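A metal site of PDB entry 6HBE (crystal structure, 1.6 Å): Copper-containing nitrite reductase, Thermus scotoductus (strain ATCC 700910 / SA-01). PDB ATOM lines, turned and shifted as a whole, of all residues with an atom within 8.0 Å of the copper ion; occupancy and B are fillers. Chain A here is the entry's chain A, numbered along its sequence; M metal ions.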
ATOM      1  N   HIS A 120     -18.478  15.842  14.676  1.00  0.00           N
ATOM      2  CA  HIS A 120     -17.756  15.005  15.635  1.00  0.00           C
ATOM      3  C   HIS A 120     -18.519  14.817  16.935  1.00  0.00           C
ATOM      4  O   HIS A 120     -18.509  13.714  17.532  1.00  0.00           O
ATOM      5  CB  HIS A 120     -16.373  15.663  15.885  1.00  0.00           C
ATOM      6  CG  HIS A 120     -15.481  14.925  16.856  1.00  0.00           C
ATOM      7  ND1 HIS A 120     -14.704  13.849  16.463  1.00  0.00           N
ATOM      8  CD2 HIS A 120     -15.165  15.167  18.153  1.00  0.00           C
ATOM      9  CE1 HIS A 120     -13.997  13.415  17.502  1.00  0.00           C
ATOM     10  NE2 HIS A 120     -14.259  14.206  18.538  1.00  0.00           N
ATOM     11  N   MET A 353      -4.491  13.095  21.573  1.00  0.00           N
ATOM     12  CA  MET A 353      -5.846  13.610  21.689  1.00  0.00           C
ATOM     13  C   MET A 353      -6.718  12.613  20.960  1.00  0.00           C
ATOM     14  O   MET A 353      -6.505  12.396  19.780  1.00  0.00           O
ATOM     15  CB  MET A 353      -5.961  15.005  21.096  1.00  0.00           C
ATOM     16  CG  MET A 353      -5.029  16.034  21.745  1.00  0.00           C
ATOM     17  SD  MET A 353      -4.214  17.030  20.487  1.00  0.00           S
ATOM     18  CE  MET A 353      -3.689  18.441  21.469  1.00  0.00           C
ATOM     19  N   ASN A 356     -12.146  13.046  22.321  1.00  0.00           N
ATOM     20  CA  ASN A 356     -12.289  14.206  23.216  1.00  0.00           C
ATOM     21  C   ASN A 356     -11.657  13.952  24.620  1.00  0.00           C
ATOM     22  O   ASN A 356     -12.251  14.233  25.672  1.00  0.00           O
ATOM     23  CB  ASN A 356     -13.766  14.632  23.299  1.00  0.00           C
ATOM     24  CG  ASN A 356     -14.240  15.371  22.062  1.00  0.00           C
ATOM     25  OD1 ASN A 356     -13.602  15.334  21.007  1.00  0.00           O
ATOM     26  ND2 ASN A 356     -15.369  16.079  22.195  1.00  0.00           N
ATOM     27  N   SER A 357     -10.446  13.402  24.600  1.00  0.00           N
ATOM     28  CA  SER A 357      -9.686  13.103  25.813  1.00  0.00           C
ATOM     29  C   SER A 357      -8.184  13.087  25.541  1.00  0.00           C
ATOM     30  O   SER A 357      -7.763  13.010  24.395  1.00  0.00           O
ATOM     31  CB  SER A 357     -10.158  11.765  26.429  1.00  0.00           C
ATOM     32  OG  SER A 357      -9.619  10.599  25.831  1.00  0.00           O
ATOM     33  N   PHE A 358      -7.372  13.164  26.607  1.00  0.00           N
ATOM     34  CA  PHE A 358      -5.919  13.035  26.486  1.00  0.00           C
ATOM     35  C   PHE A 358      -5.449  11.681  27.011  1.00  0.00           C
ATOM     36  O   PHE A 358      -5.852  11.267  28.100  1.00  0.00           O
ATOM     37  CB  PHE A 358      -5.197  14.169  27.254  1.00  0.00           C
ATOM     38  CG  PHE A 358      -5.564  15.556  26.812  1.00  0.00           C
ATOM     39  CD1 PHE A 358      -5.046  16.090  25.636  1.00  0.00           C
ATOM     40  CD2 PHE A 358      -6.403  16.348  27.581  1.00  0.00           C
ATOM     41  CE1 PHE A 358      -5.350  17.384  25.254  1.00  0.00           C
ATOM     42  CE2 PHE A 358      -6.731  17.635  27.198  1.00  0.00           C
ATOM     43  CZ  PHE A 358      -6.200  18.154  26.025  1.00  0.00           C
ATOM     44  N   ASN A 375      -2.945  14.719  17.372  1.00  0.00           N
ATOM     45  CA  ASN A 375      -4.406  14.609  17.292  1.00  0.00           C
ATOM     46  C   ASN A 375      -4.851  13.384  16.480  1.00  0.00           C
ATOM     47  O   ASN A 375      -4.731  13.372  15.253  1.00  0.00           O
ATOM     48  CB  ASN A 375      -5.068  15.880  16.736  1.00  0.00           C
ATOM     49  CG  ASN A 375      -6.593  15.865  16.917  1.00  0.00           C
ATOM     50  OD1 ASN A 375      -7.124  14.935  17.517  1.00  0.00           O
ATOM     51  ND2 ASN A 375      -7.271  16.896  16.443  1.00  0.00           N
ATOM     52  N   ASP A 377      -8.102  12.264  16.706  1.00  0.00           N
ATOM     53  CA  ASP A 377      -9.494  12.473  16.203  1.00  0.00           C
ATOM     54  C   ASP A 377      -9.394  12.852  14.711  1.00  0.00           C
ATOM     55  O   ASP A 377      -8.405  13.457  14.283  1.00  0.00           O
ATOM     56  CB  ASP A 377     -10.292  13.499  17.043  1.00  0.00           C
ATOM     57  CG  ASP A 377     -10.884  12.896  18.365  1.00  0.00           C
ATOM     58  OD1 ASP A 377     -11.188  11.687  18.433  1.00  0.00           O
ATOM     59  OD2 ASP A 377     -11.058  13.630  19.354  1.00  0.00           O
ATOM     60  N   GLY A 384     -16.008  24.299  17.666  1.00  0.00           N
ATOM     61  CA  GLY A 384     -16.576  24.017  18.985  1.00  0.00           C
ATOM     62  C   GLY A 384     -16.886  22.535  19.180  1.00  0.00           C
ATOM     63  O   GLY A 384     -16.083  21.663  18.804  1.00  0.00           O
ATOM     64  N   GLU A 385     -18.083  22.235  19.711  1.00  0.00           N
ATOM     65  CA  GLU A 385     -18.483  20.833  19.942  1.00  0.00           C
ATOM     66  C   GLU A 385     -18.740  20.056  18.645  1.00  0.00           C
ATOM     67  O   GLU A 385     -18.867  18.827  18.712  1.00  0.00           O
ATOM     68  CB  GLU A 385     -19.716  20.754  20.861  1.00  0.00           C
ATOM     69  CG  GLU A 385     -19.471  21.288  22.264  1.00  0.00           C
ATOM     70  CD  GLU A 385     -18.363  20.566  23.025  1.00  0.00           C
ATOM     71  OE1 GLU A 385     -18.295  19.294  22.996  1.00  0.00           O
ATOM     72  OE2 GLU A 385     -17.585  21.276  23.707  1.00  0.00           O
ATOM     73  N   THR A 387     -16.496  20.052  16.114  1.00  0.00           N
ATOM     74  CA  THR A 387     -15.181  19.672  15.557  1.00  0.00           C
ATOM     75  C   THR A 387     -14.418  18.721  16.464  1.00  0.00           C
ATOM     76  O   THR A 387     -14.623  18.706  17.672  1.00  0.00           O
ATOM     77  CB  THR A 387     -14.287  20.919  15.293  1.00  0.00           C
ATOM     78  OG1 THR A 387     -13.226  20.574  14.385  1.00  0.00           O
ATOM     79  CG2 THR A 387     -13.659  21.478  16.583  1.00  0.00           C
ATOM     80  N   GLY A 388     -13.524  17.937  15.854  1.00  0.00           N
ATOM     81  CA  GLY A 388     -12.540  17.096  16.532  1.00  0.00           C
ATOM     82  C   GLY A 388     -11.120  17.674  16.512  1.00  0.00           C
ATOM     83  O   GLY A 388     -10.173  16.964  16.883  1.00  0.00           O
ATOM     84  N   ARG A 389     -10.973  18.921  16.082  1.00  0.00           N
ATOM     85  CA  ARG A 389      -9.732  19.703  16.351  1.00  0.00           C
ATOM     86  C   ARG A 389      -9.542  19.945  17.867  1.00  0.00           C
ATOM     87  O   ARG A 389     -10.527  20.092  18.595  1.00  0.00           O
ATOM     88  CB  ARG A 389      -9.759  21.058  15.625  1.00  0.00           C
ATOM     89  CG  ARG A 389      -9.582  20.969  14.116  1.00  0.00           C
ATOM     90  CD  ARG A 389      -9.230  22.311  13.458  1.00  0.00           C
ATOM     91  NE  ARG A 389     -10.007  23.347  14.110  1.00  0.00           N
ATOM     92  CZ  ARG A 389     -11.277  23.675  13.854  1.00  0.00           C
ATOM     93  NH1 ARG A 389     -11.873  24.633  14.576  1.00  0.00           N
ATOM     94  NH2 ARG A 389     -11.958  23.106  12.859  1.00  0.00           N
ATOM     95  N   HIS A 390      -8.273  19.996  18.327  1.00  0.00           N
ATOM     96  CA  HIS A 390      -7.946  20.172  19.752  1.00  0.00           C
ATOM     97  C   HIS A 390      -6.633  20.930  19.940  1.00  0.00           C
ATOM     98  O   HIS A 390      -5.745  20.892  19.073  1.00  0.00           O
ATOM     99  CB  HIS A 390      -7.727  18.859  20.502  1.00  0.00           C
ATOM    100  CG  HIS A 390      -8.850  17.899  20.405  1.00  0.00           C
ATOM    101  ND1 HIS A 390     -10.040  18.103  21.061  1.00  0.00           N
ATOM    102  CD2 HIS A 390      -8.967  16.711  19.766  1.00  0.00           C
ATOM    103  CE1 HIS A 390     -10.862  17.105  20.784  1.00  0.00           C
ATOM    104  NE2 HIS A 390     -10.233  16.247  20.013  1.00  0.00           N
ATOM    105  N   ASP A 391      -6.520  21.543  21.108  1.00  0.00           N
ATOM    106  CA  ASP A 391      -5.233  22.083  21.597  1.00  0.00           C
ATOM    107  C   ASP A 391      -5.007  21.595  23.022  1.00  0.00           C
ATOM    108  O   ASP A 391      -5.816  20.831  23.586  1.00  0.00           O
ATOM    109  CB  ASP A 391      -5.197  23.607  21.451  1.00  0.00           C
ATOM    110  CG  ASP A 391      -6.249  24.324  22.291  1.00  0.00           C
ATOM    111  OD1 ASP A 391      -6.756  23.764  23.281  1.00  0.00           O
ATOM    112  OD2 ASP A 391      -6.546  25.498  21.951  1.00  0.00           O
ATOM    113  N   ALA A 392      -3.880  22.002  23.598  1.00  0.00           N
ATOM    114  CA  ALA A 392      -3.583  21.714  24.970  1.00  0.00           C
ATOM    115  C   ALA A 392      -2.945  22.975  25.575  1.00  0.00           C
ATOM    116  O   ALA A 392      -1.949  23.465  25.047  1.00  0.00           O
ATOM    117  CB  ALA A 392      -2.645  20.526  25.064  1.00  0.00           C
ATOM    118  N   LEU A 408      -4.636  21.659  16.625  1.00  0.00           N
ATOM    119  CA  LEU A 408      -4.191  20.616  15.726  1.00  0.00           C
ATOM    120  C   LEU A 408      -5.378  19.970  15.013  1.00  0.00           C
ATOM    121  O   LEU A 408      -6.341  19.585  15.670  1.00  0.00           O
ATOM    122  CB  LEU A 408      -3.417  19.551  16.524  1.00  0.00           C
ATOM    123  CG  LEU A 408      -2.205  20.069  17.340  1.00  0.00           C
ATOM    124  CD1 LEU A 408      -1.532  18.920  18.060  1.00  0.00           C
ATOM    125  CD2 LEU A 408      -1.201  20.799  16.450  1.00  0.00           C
ATOM    126  N   ILE A 427      -5.897  21.812  29.753  1.00  0.00           N
ATOM    127  CA  ILE A 427      -7.202  21.542  29.105  1.00  0.00           C
ATOM    128  C   ILE A 427      -7.129  21.814  27.608  1.00  0.00           C
ATOM    129  O   ILE A 427      -6.136  22.355  27.129  1.00  0.00           O
ATOM    130  CB  ILE A 427      -8.344  22.394  29.724  1.00  0.00           C
ATOM    131  CG1 ILE A 427      -8.112  23.894  29.497  1.00  0.00           C
ATOM    132  CG2 ILE A 427      -8.475  22.100  31.225  1.00  0.00           C
ATOM    133  CD1 ILE A 427      -9.354  24.748  29.532  1.00  0.00           C
ATOM    134  N   CYS A 428      -8.188  21.432  26.899  1.00  0.00           N
ATOM    135  CA  CYS A 428      -8.447  21.897  25.545  1.00  0.00           C
ATOM    136  C   CYS A 428      -9.318  23.152  25.589  1.00  0.00           C
ATOM    137  O   CYS A 428     -10.386  23.132  26.226  1.00  0.00           O
ATOM    138  CB  CYS A 428      -9.162  20.812  24.731  1.00  0.00           C
ATOM    139  SG  CYS A 428      -9.544  21.319  23.030  1.00  0.00           S
ATOM    140  N   SER A 429      -8.888  24.233  24.920  1.00  0.00           N
ATOM    141  CA  SER A 429      -9.667  25.499  24.896  1.00  0.00           C
ATOM    142  C   SER A 429     -10.976  25.381  24.112  1.00  0.00           C
ATOM    143  O   SER A 429     -11.935  26.114  24.389  1.00  0.00           O
ATOM    144  CB  SER A 429      -8.853  26.696  24.402  1.00  0.00           C
ATOM    145  OG  SER A 429      -8.571  26.649  23.012  1.00  0.00           O
ATOM    146  N   ILE A 430     -11.018  24.449  23.154  1.00  0.00           N
ATOM    147  CA  ILE A 430     -12.202  24.225  22.323  1.00  0.00           C
ATOM    148  C   ILE A 430     -13.257  23.418  23.092  1.00  0.00           C
ATOM    149  O   ILE A 430     -14.431  23.759  23.023  1.00  0.00           O
ATOM    150  CB  ILE A 430     -11.851  23.530  20.987  1.00  0.00           C
ATOM    151  CG1 ILE A 430     -10.868  24.365  20.156  1.00  0.00           C
ATOM    152  CG2 ILE A 430     -13.095  23.296  20.116  1.00  0.00           C
ATOM    153  CD1 ILE A 430     -10.256  23.608  18.994  1.00  0.00           C
ATOM    154  N   HIS A 431     -12.816  22.356  23.786  1.00  0.00           N
ATOM    155  CA  HIS A 431     -13.662  21.492  24.619  1.00  0.00           C
ATOM    156  C   HIS A 431     -13.174  21.508  26.083  1.00  0.00           C
ATOM    157  O   HIS A 431     -12.371  20.655  26.503  1.00  0.00           O
ATOM    158  CB  HIS A 431     -13.624  20.039  24.057  1.00  0.00           C
ATOM    159  CG  HIS A 431     -13.766  19.958  22.572  1.00  0.00           C
ATOM    160  ND1 HIS A 431     -12.696  19.748  21.730  1.00  0.00           N
ATOM    161  CD2 HIS A 431     -14.869  20.022  21.782  1.00  0.00           C
ATOM    162  CE1 HIS A 431     -13.127  19.719  20.488  1.00  0.00           C
ATOM    163  NE2 HIS A 431     -14.434  19.878  20.490  1.00  0.00           N
ATOM    164  N   PRO A 432     -13.625  22.492  26.884  1.00  0.00           N
ATOM    165  CA  PRO A 432     -12.958  22.736  28.193  1.00  0.00           C
ATOM    166  C   PRO A 432     -13.096  21.687  29.294  1.00  0.00           C
ATOM    167  O   PRO A 432     -12.336  21.715  30.296  1.00  0.00           O
ATOM    168  CB  PRO A 432     -13.569  24.070  28.639  1.00  0.00           C
ATOM    169  CG  PRO A 432     -13.960  24.723  27.362  1.00  0.00           C
ATOM    170  CD  PRO A 432     -14.552  23.587  26.562  1.00  0.00           C
ATOM    171  N   TYR A 433     -14.009  20.741  29.105  1.00  0.00           N
ATOM    172  CA  TYR A 433     -14.091  19.526  29.954  1.00  0.00           C
ATOM    173  C   TYR A 433     -12.990  18.462  29.707  1.00  0.00           C
ATOM    174  O   TYR A 433     -12.847  17.542  30.497  1.00  0.00           O
ATOM    175  CB  TYR A 433     -15.494  18.887  29.841  1.00  0.00           C
ATOM    176  CG  TYR A 433     -15.881  18.575  28.416  1.00  0.00           C
ATOM    177  CD1 TYR A 433     -16.497  19.530  27.596  1.00  0.00           C
ATOM    178  CD2 TYR A 433     -15.600  17.329  27.868  1.00  0.00           C
ATOM    179  CE1 TYR A 433     -16.811  19.242  26.272  1.00  0.00           C
ATOM    180  CE2 TYR A 433     -15.919  17.025  26.551  1.00  0.00           C
ATOM    181  CZ  TYR A 433     -16.506  17.985  25.756  1.00  0.00           C
ATOM    182  OH  TYR A 433     -16.816  17.693  24.456  1.00  0.00           O
ATOM    183  N   MET A 434     -12.223  18.573  28.619  1.00  0.00           N
ATOM    184  CA  MET A 434     -11.040  17.713  28.402  1.00  0.00           C
ATOM    185  C   MET A 434      -9.944  18.201  29.339  1.00  0.00           C
ATOM    186  O   MET A 434      -9.681  19.398  29.362  1.00  0.00           O
ATOM    187  CB  MET A 434     -10.530  17.803  26.965  1.00  0.00           C
ATOM    188  CG  MET A 434     -11.529  17.322  25.928  1.00  0.00           C
ATOM    189  SD  MET A 434     -10.977  17.455  24.207  1.00  0.00           S
ATOM    190  CE  MET A 434      -9.361  16.731  24.179  1.00  0.00           C
HETATM  191 CU    CU M   1     -10.724  19.630  22.172  1.00  0.00          CU
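The side-chain sulfur of Cys 428 lies close to the backbone NH of Ile 430 (3.5 Å). O of Gly 388 lies close to NE2 of His 390 (3.2 Å). The side-chain sulfur (SD) of Met 434 sits close to a ring nitrogen (ND1) of His 390, 3.3 Å away. A ring nitrogen (NE2) of His 431 sits at hydrogen-bond distance from the backbone carbonyl oxygen (O) of Thr 387, at 3.1 Å. The backbone carbonyl oxygen of His 390 is in hydrogen-bond range of the backbone NH of Leu 408 (2.8 Å). The side-chain sulfur (SD) of Met 434 lies close to a ring nitrogen (ND1) of His 431. The backbone NH of Asp 391 lies close to the side-chain sulfur of Cys 428, at 3.6 Å. NE2 of His 390 sits at hydrogen-bond distance from OD2 of Asp 377, at 2.8 Å.
Merely in contact with the copper ion: Arg 389. Of the 24 residues printed, 5 come within 4 Å of the copper ion.
The copper ion is bound by ND1 of His 390 (2.0 Å), ND1 of His 431 (2.0 Å) and SG of Cys 428 (2.2 Å). The copper ion has three donor atoms within binding distance. Slightly farther from the copper ion lies SD of Met 434 (3.0 Å).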
